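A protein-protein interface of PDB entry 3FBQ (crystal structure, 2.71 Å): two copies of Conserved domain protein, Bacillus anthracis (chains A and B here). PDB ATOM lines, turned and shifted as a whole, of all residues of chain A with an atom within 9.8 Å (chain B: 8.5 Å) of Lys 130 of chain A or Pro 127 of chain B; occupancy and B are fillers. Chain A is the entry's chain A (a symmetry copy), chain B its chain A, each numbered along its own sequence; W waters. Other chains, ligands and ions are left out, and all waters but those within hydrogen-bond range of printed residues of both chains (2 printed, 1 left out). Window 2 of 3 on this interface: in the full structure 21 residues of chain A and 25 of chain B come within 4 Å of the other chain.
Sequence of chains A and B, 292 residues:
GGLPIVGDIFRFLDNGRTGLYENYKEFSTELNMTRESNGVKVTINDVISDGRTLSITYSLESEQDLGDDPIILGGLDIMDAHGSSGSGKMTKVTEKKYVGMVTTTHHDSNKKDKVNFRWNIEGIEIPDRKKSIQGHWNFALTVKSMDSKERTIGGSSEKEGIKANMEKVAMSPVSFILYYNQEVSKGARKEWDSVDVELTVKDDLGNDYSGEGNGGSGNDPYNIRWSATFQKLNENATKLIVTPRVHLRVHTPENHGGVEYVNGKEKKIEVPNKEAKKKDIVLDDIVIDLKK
OE2 of Glu 125 of chain A sits close to OE1 of Glu 125 of chain B (2.7 Å).
The backbone carbonyl oxygen (O) of Ile 72 of chain B lies close to the side-chain amide oxygen (OE1) of Gln 134 of chain A (3.3 Å).
The side-chain amide oxygen (OE1) of Gln 64 of chain A is in hydrogen-bond range of the side-chain amino group (NZ) of Lys 131 of chain A, at 3.3 Å.
N of Ile 71 of chain B is in hydrogen-bond range of O of Glu 125 of chain B (2.9 Å).
The backbone NH of Ile 126 of chain A lies within hydrogen-bond range of the backbone carbonyl oxygen of Lys 131 of chain A, at 2.7 Å.
Among the printed residues, pairs that only touch across the chains: Glu 125 of chain A with Ile 71 of chain B, Ser 132 of chain A with Ile 71 of chain B, Lys 130 of chain A with Asp 69 of chain B, Lys 130 of chain A with Pro 127 of chain B and Lys 131 of chain A with Ile 71 of chain B.
Asp 128 of chain A touches none of the printed residues of chain B.
Of chain B, only Asp 69 (3.5 Å) and Pro 127 (3.7 Å) come within 4 Å of Lys 130 of chain A.
Of the printed residues of chain B, Lys 131 of chain A touches Ile 71.
Of the printed residues of chain B, Gln 134 of chain A touches Ile 72 (3.3 Å).
Asp 69 of chain B touches just one residue of chain A: Lys 130 (3.5 Å).
Glu 125 of chain B touches one residue of chain A.
Pro 127 of chain B touches one residue of chain A.
Asp 128 of chain B touches none of the printed residues of chain A.
Lys 130 of chain B touches none of the printed residues of chain A.
Of the 19 printed residues of chain A, 5 touch a printed residue of chain B.
Printed residues of chain A that touch a printed residue of chain B: Glu 125, Lys 130, Lys 131, Ser 132 and Gln 134.
Hydrophobic or aromatic side chains of chain B that line the printed part of chain A: Ile 71, Ile 72 and Pro 127.
Among the printed residues, 7 pairs touch across the chains.
Among the printed residues, no Asp or Glu carboxylate lies within 4 Å of a Lys or Arg side-chain nitrogen of the other chain.
Glu 125 of chain A touches its own counterpart, Glu 125 of chain B.
Lys 130 of chain A touches Asp 69 of chain B, but with the chains exchanged Asp 69 of chain A does not touch Lys 130 of chain B (12.6 Å).
Lys 130 of chain A touches Pro 127 of chain B, but with the chains exchanged Pro 127 of chain A does not touch Lys 130 of chain B (8.3 Å).
Water W1 lies within hydrogen-bond range of O of Lys 130 of chain A (2.6 Å), OD1 of Asp 128 of chain B (3.0 Å) and N of Asp 69 of chain B (3.2 Å).
Water W2 lies within hydrogen-bond range of N of Ile 72 of chain B (2.9 Å) and NE2 of Gln 134 of chain A (3.2 Å).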
ATOM      1  N   GLN A  64     -17.616  15.500  -5.831  1.00  0.00           N
ATOM      2  CA  GLN A  64     -17.411  14.062  -5.960  1.00  0.00           C
ATOM      3  C   GLN A  64     -18.695  13.293  -5.669  1.00  0.00           C
ATOM      4  O   GLN A  64     -19.475  13.675  -4.797  1.00  0.00           O
ATOM      5  CB  GLN A  64     -16.295  13.595  -5.021  1.00  0.00           C
ATOM      6  CG  GLN A  64     -16.731  13.422  -3.576  1.00  0.00           C
ATOM      7  CD  GLN A  64     -16.504  12.014  -3.063  1.00  0.00           C
ATOM      8  OE1 GLN A  64     -15.560  11.337  -3.471  1.00  0.00           O
ATOM      9  NE2 GLN A  64     -17.371  11.563  -2.164  1.00  0.00           N
ATOM     10  N   ASP A  65     -18.908  12.208  -6.406  1.00  0.00           N
ATOM     11  CA  ASP A  65     -20.249  11.673  -6.612  1.00  0.00           C
ATOM     12  C   ASP A  65     -20.850  11.173  -5.304  1.00  0.00           C
ATOM     13  O   ASP A  65     -20.220  10.410  -4.571  1.00  0.00           O
ATOM     14  CB  ASP A  65     -20.223  10.544  -7.645  1.00  0.00           C
ATOM     15  CG  ASP A  65     -20.652  11.006  -9.024  1.00  0.00           C
ATOM     16  OD1 ASP A  65     -20.058  11.977  -9.539  1.00  0.00           O
ATOM     17  OD2 ASP A  65     -21.583  10.398  -9.592  1.00  0.00           O
ATOM     18  N   LEU A  66     -22.074  11.606  -5.016  1.00  0.00           N
ATOM     19  CA  LEU A  66     -22.878  10.990  -3.967  1.00  0.00           C
ATOM     20  C   LEU A  66     -23.563   9.724  -4.470  1.00  0.00           C
ATOM     21  O   LEU A  66     -23.992   8.883  -3.680  1.00  0.00           O
ATOM     22  CB  LEU A  66     -23.920  11.979  -3.441  1.00  0.00           C
ATOM     23  CG  LEU A  66     -23.401  13.082  -2.517  1.00  0.00           C
ATOM     24  CD1 LEU A  66     -22.566  12.493  -1.391  1.00  0.00           C
ATOM     25  CD2 LEU A  66     -22.602  14.110  -3.302  1.00  0.00           C
ATOM     26  N   GLY A  67     -23.661   9.594  -5.789  1.00  0.00           N
ATOM     27  CA  GLY A  67     -24.392   8.513  -6.389  1.00  0.00           C
ATOM     28  C   GLY A  67     -25.880   8.729  -6.228  1.00  0.00           C
ATOM     29  O   GLY A  67     -26.332   9.863  -6.215  1.00  0.00           O
ATOM     30  N   ASP A  68     -26.611   7.627  -6.056  1.00  0.00           N
ATOM     31  CA  ASP A  68     -28.049   7.558  -6.262  1.00  0.00           C
ATOM     32  C   ASP A  68     -28.857   7.675  -4.982  1.00  0.00           C
ATOM     33  O   ASP A  68     -29.986   8.180  -4.985  1.00  0.00           O
ATOM     34  CB  ASP A  68     -28.399   6.250  -6.990  1.00  0.00           C
ATOM     35  CG  ASP A  68     -28.454   6.429  -8.507  1.00  0.00           C
ATOM     36  OD1 ASP A  68     -29.339   7.194  -9.015  1.00  0.00           O
ATOM     37  OD2 ASP A  68     -27.600   5.838  -9.197  1.00  0.00           O
ATOM     38  N   ASP A  69     -28.297   7.196  -3.880  1.00  0.00           N
ATOM     39  CA  ASP A  69     -29.050   7.241  -2.643  1.00  0.00           C
ATOM     40  C   ASP A  69     -28.126   7.498  -1.460  1.00  0.00           C
ATOM     41  O   ASP A  69     -27.898   6.591  -0.631  1.00  0.00           O
ATOM     42  CB  ASP A  69     -29.857   5.948  -2.423  1.00  0.00           C
ATOM     43  CG  ASP A  69     -31.274   6.046  -2.929  1.00  0.00           C
ATOM     44  OD1 ASP A  69     -31.936   7.053  -2.600  1.00  0.00           O
ATOM     45  OD2 ASP A  69     -31.737   5.113  -3.637  1.00  0.00           O
ATOM     46  N   PRO A  70     -27.623   8.740  -1.359  1.00  0.00           N
ATOM     47  CA  PRO A  70     -26.703   9.003  -0.244  1.00  0.00           C
ATOM     48  C   PRO A  70     -27.431   8.869   1.112  1.00  0.00           C
ATOM     49  O   PRO A  70     -28.621   9.146   1.211  1.00  0.00           O
ATOM     50  CB  PRO A  70     -26.196  10.432  -0.515  1.00  0.00           C
ATOM     51  CG  PRO A  70     -26.797  10.868  -1.929  1.00  0.00           C
ATOM     52  CD  PRO A  70     -27.886   9.900  -2.249  1.00  0.00           C
ATOM     53  N   LEU A  73     -25.983  10.260   7.864  1.00  0.00           N
ATOM     54  CA  LEU A  73     -25.763   9.795   9.219  1.00  0.00           C
ATOM     55  C   LEU A  73     -25.801  10.961  10.236  1.00  0.00           C
ATOM     56  O   LEU A  73     -24.964  11.899  10.154  1.00  0.00           O
ATOM     57  CB  LEU A  73     -24.418   9.065   9.323  1.00  0.00           C
ATOM     58  CG  LEU A  73     -24.167   7.849   8.426  1.00  0.00           C
ATOM     59  CD1 LEU A  73     -22.744   7.311   8.351  1.00  0.00           C
ATOM     60  CD2 LEU A  73     -25.176   6.719   8.636  1.00  0.00           C
ATOM     61  N   ILE A 124     -21.823  11.021   5.570  1.00  0.00           N
ATOM     62  CA  ILE A 124     -22.586  10.785   4.353  1.00  0.00           C
ATOM     63  C   ILE A 124     -22.105   9.472   3.853  1.00  0.00           C
ATOM     64  O   ILE A 124     -20.935   9.341   3.467  1.00  0.00           O
ATOM     65  CB  ILE A 124     -22.226  11.798   3.265  1.00  0.00           C
ATOM     66  CG1 ILE A 124     -22.306  13.207   3.850  1.00  0.00           C
ATOM     67  CG2 ILE A 124     -23.202  11.679   2.140  1.00  0.00           C
ATOM     68  CD1 ILE A 124     -23.716  13.582   4.365  1.00  0.00           C
ATOM     69  N   GLU A 125     -22.965   8.481   3.881  1.00  0.00           N
ATOM     70  CA  GLU A 125     -22.589   7.221   3.272  1.00  0.00           C
ATOM     71  C   GLU A 125     -22.936   7.388   1.833  1.00  0.00           C
ATOM     72  O   GLU A 125     -23.884   8.095   1.508  1.00  0.00           O
ATOM     73  CB  GLU A 125     -23.457   6.114   3.752  1.00  0.00           C
ATOM     74  CG  GLU A 125     -23.050   5.451   4.969  1.00  0.00           C
ATOM     75  CD  GLU A 125     -23.527   4.029   4.903  1.00  0.00           C
ATOM     76  OE1 GLU A 125     -24.652   3.781   5.362  1.00  0.00           O
ATOM     77  OE2 GLU A 125     -22.852   3.170   4.305  1.00  0.00           O
ATOM     78  N   ILE A 126     -22.160   6.734   0.987  1.00  0.00           N
ATOM     79  CA  ILE A 126     -22.347   6.690  -0.444  1.00  0.00           C
ATOM     80  C   ILE A 126     -22.383   5.204  -0.690  1.00  0.00           C
ATOM     81  O   ILE A 126     -21.344   4.529  -0.940  1.00  0.00           O
ATOM     82  CB  ILE A 126     -21.167   7.279  -1.206  1.00  0.00           C
ATOM     83  CG1 ILE A 126     -20.963   8.759  -0.829  1.00  0.00           C
ATOM     84  CG2 ILE A 126     -21.401   7.095  -2.673  1.00  0.00           C
ATOM     85  CD1 ILE A 126     -19.509   9.177  -0.661  1.00  0.00           C
ATOM     86  N   PRO A 127     -23.589   4.660  -0.578  1.00  0.00           N
ATOM     87  CA  PRO A 127     -23.628   3.226  -0.742  1.00  0.00           C
ATOM     88  C   PRO A 127     -23.135   2.849  -2.153  1.00  0.00           C
ATOM     89  O   PRO A 127     -22.434   1.846  -2.287  1.00  0.00           O
ATOM     90  CB  PRO A 127     -25.090   2.902  -0.496  1.00  0.00           C
ATOM     91  CG  PRO A 127     -25.572   4.022   0.387  1.00  0.00           C
ATOM     92  CD  PRO A 127     -24.885   5.223  -0.186  1.00  0.00           C
ATOM     93  N   ASP A 128     -23.455   3.634  -3.201  1.00  0.00           N
ATOM     94  CA  ASP A 128     -22.994   3.250  -4.569  1.00  0.00           C
ATOM     95  C   ASP A 128     -21.495   2.963  -4.513  1.00  0.00           C
ATOM     96  O   ASP A 128     -21.070   1.937  -4.957  1.00  0.00           O
ATOM     97  CB  ASP A 128     -23.283   4.324  -5.629  1.00  0.00           C
ATOM     98  CG  ASP A 128     -24.762   4.423  -6.000  1.00  0.00           C
ATOM     99  OD1 ASP A 128     -25.629   3.958  -5.220  1.00  0.00           O
ATOM    100  OD2 ASP A 128     -25.068   4.985  -7.088  1.00  0.00           O
ATOM    101  N   ARG A 129     -20.710   3.852  -3.902  1.00  0.00           N
ATOM    102  CA  ARG A 129     -19.263   3.697  -3.852  1.00  0.00           C
ATOM    103  C   ARG A 129     -18.694   3.105  -2.549  1.00  0.00           C
ATOM    104  O   ARG A 129     -17.519   3.221  -2.301  1.00  0.00           O
ATOM    105  CB  ARG A 129     -18.608   5.029  -4.205  1.00  0.00           C
ATOM    106  CG  ARG A 129     -17.479   4.862  -5.257  1.00  0.00           C
ATOM    107  CD  ARG A 129     -17.667   5.732  -6.532  1.00  0.00           C
ATOM    108  NE  ARG A 129     -19.031   6.263  -6.693  1.00  0.00           N
ATOM    109  CZ  ARG A 129     -20.128   5.558  -7.026  1.00  0.00           C
ATOM    110  NH1 ARG A 129     -20.052   4.234  -7.236  1.00  0.00           N
ATOM    111  NH2 ARG A 129     -21.315   6.183  -7.156  1.00  0.00           N
ATOM    112  N   LYS A 130     -19.548   2.513  -1.701  1.00  0.00           N
ATOM    113  CA  LYS A 130     -19.143   1.561  -0.621  1.00  0.00           C
ATOM    114  C   LYS A 130     -18.366   2.174   0.575  1.00  0.00           C
ATOM    115  O   LYS A 130     -17.542   1.540   1.231  1.00  0.00           O
ATOM    116  CB  LYS A 130     -18.317   0.455  -1.269  1.00  0.00           C
ATOM    117  CG  LYS A 130     -18.602  -0.935  -0.777  1.00  0.00           C
ATOM    118  CD  LYS A 130     -19.843  -1.460  -1.393  1.00  0.00           C
ATOM    119  CE  LYS A 130     -19.707  -2.929  -1.584  1.00  0.00           C
ATOM    120  NZ  LYS A 130     -19.351  -3.314  -2.986  1.00  0.00           N
ATOM    121  N   LYS A 131     -18.721   3.401   0.878  1.00  0.00           N
ATOM    122  CA  LYS A 131     -17.819   4.393   1.369  1.00  0.00           C
ATOM    123  C   LYS A 131     -18.675   5.411   2.086  1.00  0.00           C
ATOM    124  O   LYS A 131     -19.880   5.496   1.814  1.00  0.00           O
ATOM    125  CB  LYS A 131     -17.244   5.108   0.165  1.00  0.00           C
ATOM    126  CG  LYS A 131     -15.903   5.633   0.429  1.00  0.00           C
ATOM    127  CD  LYS A 131     -15.481   6.512  -0.703  1.00  0.00           C
ATOM    128  CE  LYS A 131     -16.161   7.837  -0.604  1.00  0.00           C
ATOM    129  NZ  LYS A 131     -15.991   8.463  -1.922  1.00  0.00           N
ATOM    130  N   SER A 132     -18.064   6.195   2.974  1.00  0.00           N
ATOM    131  CA  SER A 132     -18.774   7.290   3.615  1.00  0.00           C
ATOM    132  C   SER A 132     -17.789   8.420   3.627  1.00  0.00           C
ATOM    133  O   SER A 132     -16.601   8.166   3.484  1.00  0.00           O
ATOM    134  CB  SER A 132     -19.161   6.957   5.035  1.00  0.00           C
ATOM    135  OG  SER A 132     -17.984   6.605   5.751  1.00  0.00           O
ATOM    136  N   ILE A 133     -18.312   9.649   3.733  1.00  0.00           N
ATOM    137  CA  ILE A 133     -17.509  10.799   4.033  1.00  0.00           C
ATOM    138  C   ILE A 133     -17.720  11.106   5.519  1.00  0.00           C
ATOM    139  O   ILE A 133     -18.826  11.451   5.960  1.00  0.00           O
ATOM    140  CB  ILE A 133     -17.846  12.012   3.139  1.00  0.00           C
ATOM    141  CG1 ILE A 133     -17.449  11.781   1.689  1.00  0.00           C
ATOM    142  CG2 ILE A 133     -17.100  13.253   3.594  1.00  0.00           C
ATOM    143  CD1 ILE A 133     -18.416  12.426   0.796  1.00  0.00           C
ATOM    144  N   GLN A 134     -16.657  10.945   6.295  1.00  0.00           N
ATOM    145  CA  GLN A 134     -16.688  11.248   7.715  1.00  0.00           C
ATOM    146  C   GLN A 134     -16.590  12.748   7.998  1.00  0.00           C
ATOM    147  O   GLN A 134     -15.934  13.470   7.274  1.00  0.00           O
ATOM    148  CB  GLN A 134     -15.528  10.523   8.370  1.00  0.00           C
ATOM    149  CG  GLN A 134     -15.673   8.999   8.281  1.00  0.00           C
ATOM    150  CD  GLN A 134     -16.618   8.400   9.331  1.00  0.00           C
ATOM    151  OE1 GLN A 134     -17.742   7.929   9.023  1.00  0.00           O
ATOM    152  NE2 GLN A 134     -16.136   8.380  10.593  1.00  0.00           N
ATOM    153  N   ASP B  65     -13.240  -9.982   9.030  1.00  0.00           N
ATOM    154  CA  ASP B  65     -12.804  -9.000   8.046  1.00  0.00           C
ATOM    155  C   ASP B  65     -13.624  -7.718   8.144  1.00  0.00           C
ATOM    156  O   ASP B  65     -14.853  -7.756   8.159  1.00  0.00           O
ATOM    157  CB  ASP B  65     -12.901  -9.578   6.632  1.00  0.00           C
ATOM    158  CG  ASP B  65     -11.565 -10.070   6.111  1.00  0.00           C
ATOM    159  OD1 ASP B  65     -10.927 -10.898   6.794  1.00  0.00           O
ATOM    160  OD2 ASP B  65     -11.153  -9.628   5.018  1.00  0.00           O
ATOM    161  N   LEU B  66     -12.934  -6.583   8.211  1.00  0.00           N
ATOM    162  CA  LEU B  66     -13.571  -5.287   8.013  1.00  0.00           C
ATOM    163  C   LEU B  66     -13.733  -4.973   6.530  1.00  0.00           C
ATOM    164  O   LEU B  66     -14.535  -4.121   6.149  1.00  0.00           O
ATOM    165  CB  LEU B  66     -12.763  -4.184   8.699  1.00  0.00           C
ATOM    166  CG  LEU B  66     -12.880  -4.106  10.223  1.00  0.00           C
ATOM    167  CD1 LEU B  66     -14.338  -4.085  10.651  1.00  0.00           C
ATOM    168  CD2 LEU B  66     -12.141  -5.263  10.878  1.00  0.00           C
ATOM    169  N   GLY B  67     -12.965  -5.668   5.696  1.00  0.00           N
ATOM    170  CA  GLY B  67     -12.929  -5.384   4.289  1.00  0.00           C
ATOM    171  C   GLY B  67     -12.173  -4.101   4.029  1.00  0.00           C
ATOM    172  O   GLY B  67     -11.247  -3.783   4.759  1.00  0.00           O
ATOM    173  N   ASP B  68     -12.618  -3.359   3.015  1.00  0.00           N
ATOM    174  CA  ASP B  68     -11.842  -2.320   2.357  1.00  0.00           C
ATOM    175  C   ASP B  68     -12.155  -0.919   2.848  1.00  0.00           C
ATOM    176  O   ASP B  68     -11.290  -0.034   2.849  1.00  0.00           O
ATOM    177  CB  ASP B  68     -12.055  -2.407   0.837  1.00  0.00           C
ATOM    178  CG  ASP B  68     -10.995  -3.269   0.153  1.00  0.00           C
ATOM    179  OD1 ASP B  68      -9.776  -2.893   0.170  1.00  0.00           O
ATOM    180  OD2 ASP B  68     -11.360  -4.337  -0.377  1.00  0.00           O
ATOM    181  N   ASP B  69     -13.397  -0.694   3.254  1.00  0.00           N
ATOM    182  CA  ASP B  69     -13.757   0.641   3.686  1.00  0.00           C
ATOM    183  C   ASP B  69     -14.759   0.585   4.830  1.00  0.00           C
ATOM    184  O   ASP B  69     -15.945   0.935   4.646  1.00  0.00           O
ATOM    185  CB  ASP B  69     -14.316   1.482   2.523  1.00  0.00           C
ATOM    186  CG  ASP B  69     -13.262   2.318   1.842  1.00  0.00           C
ATOM    187  OD1 ASP B  69     -12.507   2.999   2.570  1.00  0.00           O
ATOM    188  OD2 ASP B  69     -13.196   2.316   0.585  1.00  0.00           O
ATOM    189  N   PRO B  70     -14.281   0.181   6.019  1.00  0.00           N
ATOM    190  CA  PRO B  70     -15.237   0.088   7.131  1.00  0.00           C
ATOM    191  C   PRO B  70     -15.793   1.482   7.495  1.00  0.00           C
ATOM    192  O   PRO B  70     -15.104   2.486   7.353  1.00  0.00           O
ATOM    193  CB  PRO B  70     -14.416  -0.548   8.269  1.00  0.00           C
ATOM    194  CG  PRO B  70     -12.992  -0.921   7.650  1.00  0.00           C
ATOM    195  CD  PRO B  70     -12.881  -0.188   6.356  1.00  0.00           C
ATOM    196  N   ILE B  71     -17.040   1.561   7.938  1.00  0.00           N
ATOM    197  CA  ILE B  71     -17.603   2.856   8.304  1.00  0.00           C
ATOM    198  C   ILE B  71     -17.858   2.993   9.815  1.00  0.00           C
ATOM    199  O   ILE B  71     -18.644   2.223  10.400  1.00  0.00           O
ATOM    200  CB  ILE B  71     -18.914   3.079   7.586  1.00  0.00           C
ATOM    201  CG1 ILE B  71     -18.720   2.929   6.105  1.00  0.00           C
ATOM    202  CG2 ILE B  71     -19.429   4.478   7.849  1.00  0.00           C
ATOM    203  CD1 ILE B  71     -19.801   3.564   5.368  1.00  0.00           C
ATOM    204  N   ILE B  72     -17.173   3.942  10.455  1.00  0.00           N
ATOM    205  CA  ILE B  72     -17.396   4.185  11.880  1.00  0.00           C
ATOM    206  C   ILE B  72     -18.732   4.887  12.013  1.00  0.00           C
ATOM    207  O   ILE B  72     -18.837   6.021  11.513  1.00  0.00           O
ATOM    208  CB  ILE B  72     -16.393   5.190  12.539  1.00  0.00           C
ATOM    209  CG1 ILE B  72     -14.923   4.740  12.469  1.00  0.00           C
ATOM    210  CG2 ILE B  72     -16.779   5.367  14.018  1.00  0.00           C
ATOM    211  CD1 ILE B  72     -14.667   3.337  13.165  1.00  0.00           C
ATOM    212  N   ILE B 124     -19.855  -0.497  13.458  1.00  0.00           N
ATOM    213  CA  ILE B 124     -18.895  -0.591  12.367  1.00  0.00           C
ATOM    214  C   ILE B 124     -19.652  -1.212  11.250  1.00  0.00           C
ATOM    215  O   ILE B 124     -20.065  -2.376  11.348  1.00  0.00           O
ATOM    216  CB  ILE B 124     -17.770  -1.572  12.699  1.00  0.00           C
ATOM    217  CG1 ILE B 124     -17.197  -1.228  14.073  1.00  0.00           C
ATOM    218  CG2 ILE B 124     -16.689  -1.446  11.674  1.00  0.00           C
ATOM    219  CD1 ILE B 124     -16.592   0.193  14.151  1.00  0.00           C
ATOM    220  N   GLU B 125     -19.878  -0.457  10.201  1.00  0.00           N
ATOM    221  CA  GLU B 125     -20.484  -1.060   9.031  1.00  0.00           C
ATOM    222  C   GLU B 125     -19.337  -1.640   8.279  1.00  0.00           C
ATOM    223  O   GLU B 125     -18.236  -1.102   8.327  1.00  0.00           O
ATOM    224  CB  GLU B 125     -21.054  -0.026   8.130  1.00  0.00           C
ATOM    225  CG  GLU B 125     -22.408   0.398   8.401  1.00  0.00           C
ATOM    226  CD  GLU B 125     -23.034   0.810   7.101  1.00  0.00           C
ATOM    227  OE1 GLU B 125     -22.926   1.999   6.764  1.00  0.00           O
ATOM    228  OE2 GLU B 125     -23.539  -0.047   6.350  1.00  0.00           O
ATOM    229  N   ILE B 126     -19.610  -2.734   7.591  1.00  0.00           N
ATOM    230  CA  ILE B 126     -18.679  -3.428   6.733  1.00  0.00           C
ATOM    231  C   ILE B 126     -19.449  -3.474   5.439  1.00  0.00           C
ATOM    232  O   ILE B 126     -20.225  -4.427   5.141  1.00  0.00           O
ATOM    233  CB  ILE B 126     -18.414  -4.856   7.192  1.00  0.00           C
ATOM    234  CG1 ILE B 126     -17.809  -4.867   8.609  1.00  0.00           C
ATOM    235  CG2 ILE B 126     -17.527  -5.527   6.191  1.00  0.00           C
ATOM    236  CD1 ILE B 126     -18.350  -5.958   9.521  1.00  0.00           C
ATOM    237  N   PRO B 127     -19.277  -2.411   4.661  1.00  0.00           N
ATOM    238  CA  PRO B 127     -20.063  -2.410   3.450  1.00  0.00           C
ATOM    239  C   PRO B 127     -19.681  -3.624   2.579  1.00  0.00           C
ATOM    240  O   PRO B 127     -20.572  -4.220   1.973  1.00  0.00           O
ATOM    241  CB  PRO B 127     -19.710  -1.073   2.827  1.00  0.00           C
ATOM    242  CG  PRO B 127     -19.307  -0.215   3.996  1.00  0.00           C
ATOM    243  CD  PRO B 127     -18.534  -1.163   4.859  1.00  0.00           C
ATOM    244  N   ASP B 128     -18.395  -4.023   2.522  1.00  0.00           N
ATOM    245  CA  ASP B 128     -18.029  -5.185   1.657  1.00  0.00           C
ATOM    246  C   ASP B 128     -18.968  -6.345   1.981  1.00  0.00           C
ATOM    247  O   ASP B 128     -19.551  -6.901   1.097  1.00  0.00           O
ATOM    248  CB  ASP B 128     -16.568  -5.630   1.828  1.00  0.00           C
ATOM    249  CG  ASP B 128     -15.566  -4.664   1.199  1.00  0.00           C
ATOM    250  OD1 ASP B 128     -15.914  -3.483   0.954  1.00  0.00           O
ATOM    251  OD2 ASP B 128     -14.403  -5.087   0.952  1.00  0.00           O
ATOM    252  N   ARG B 129     -19.158  -6.657   3.264  1.00  0.00           N
ATOM    253  CA  ARG B 129     -19.986  -7.785   3.669  1.00  0.00           C
ATOM    254  C   ARG B 129     -21.425  -7.444   4.097  1.00  0.00           C
ATOM    255  O   ARG B 129     -22.071  -8.250   4.723  1.00  0.00           O
ATOM    256  CB  ARG B 129     -19.248  -8.584   4.739  1.00  0.00           C
ATOM    257  CG  ARG B 129     -19.259 -10.107   4.441  1.00  0.00           C
ATOM    258  CD  ARG B 129     -17.846 -10.750   4.374  1.00  0.00           C
ATOM    259  NE  ARG B 129     -16.754  -9.773   4.230  1.00  0.00           N
ATOM    260  CZ  ARG B 129     -16.467  -9.054   3.129  1.00  0.00           C
ATOM    261  NH1 ARG B 129     -17.210  -9.177   2.019  1.00  0.00           N
ATOM    262  NH2 ARG B 129     -15.420  -8.205   3.136  1.00  0.00           N
ATOM    263  N   LYS B 130     -21.901  -6.228   3.794  1.00  0.00           N
ATOM    264  CA  LYS B 130     -23.353  -5.870   3.769  1.00  0.00           C
ATOM    265  C   LYS B 130     -24.069  -5.817   5.146  1.00  0.00           C
ATOM    266  O   LYS B 130     -25.265  -6.063   5.285  1.00  0.00           O
ATOM    267  CB  LYS B 130     -24.056  -6.866   2.852  1.00  0.00           C
ATOM    268  CG  LYS B 130     -25.094  -6.281   1.938  1.00  0.00           C
ATOM    269  CD  LYS B 130     -24.451  -5.621   0.778  1.00  0.00           C
ATOM    270  CE  LYS B 130     -25.326  -5.774  -0.415  1.00  0.00           C
ATOM    271  NZ  LYS B 130     -24.890  -6.872  -1.334  1.00  0.00           N
ATOM    272  N   LYS B 131     -23.307  -5.410   6.134  1.00  0.00           N
ATOM    273  CA  LYS B 131     -23.417  -5.892   7.474  1.00  0.00           C
ATOM    274  C   LYS B 131     -22.796  -4.827   8.348  1.00  0.00           C
ATOM    275  O   LYS B 131     -21.995  -4.022   7.855  1.00  0.00           O
ATOM    276  CB  LYS B 131     -22.512  -7.101   7.587  1.00  0.00           C
ATOM    277  CG  LYS B 131     -22.989  -8.049   8.596  1.00  0.00           C
ATOM    278  CD  LYS B 131     -21.951  -9.099   8.822  1.00  0.00           C
ATOM    279  CE  LYS B 131     -20.847  -8.556   9.667  1.00  0.00           C
ATOM    280  NZ  LYS B 131     -19.734  -9.502   9.511  1.00  0.00           N
ATOM    281  N   SER B 132     -23.136  -4.831   9.636  1.00  0.00           N
ATOM    282  CA  SER B 132     -22.492  -3.932  10.580  1.00  0.00           C
ATOM    283  C   SER B 132     -22.263  -4.770  11.802  1.00  0.00           C
ATOM    284  O   SER B 132     -22.911  -5.799  11.938  1.00  0.00           O
ATOM    285  CB  SER B 132     -23.378  -2.764  10.942  1.00  0.00           C
ATOM    286  OG  SER B 132     -24.603  -3.272  11.455  1.00  0.00           O
ATOM    287  N   ILE B 133     -21.300  -4.344  12.630  1.00  0.00           N
ATOM    288  CA  ILE B 133     -21.145  -4.867  13.957  1.00  0.00           C
ATOM    289  C   ILE B 133     -21.752  -3.833  14.909  1.00  0.00           C
ATOM    290  O   ILE B 133     -21.269  -2.699  15.030  1.00  0.00           O
ATOM    291  CB  ILE B 133     -19.674  -5.182  14.306  1.00  0.00           C
ATOM    292  CG1 ILE B 133     -19.131  -6.349  13.495  1.00  0.00           C
ATOM    293  CG2 ILE B 133     -19.529  -5.572  15.765  1.00  0.00           C
ATOM    294  CD1 ILE B 133     -17.714  -6.129  13.188  1.00  0.00           C
HETATM  295  O   HOH W   1     -16.247  -0.614   1.777  1.00  0.00           O
HETATM  296  O   HOH W   2     -15.254   5.682   9.101  1.00  0.00           O
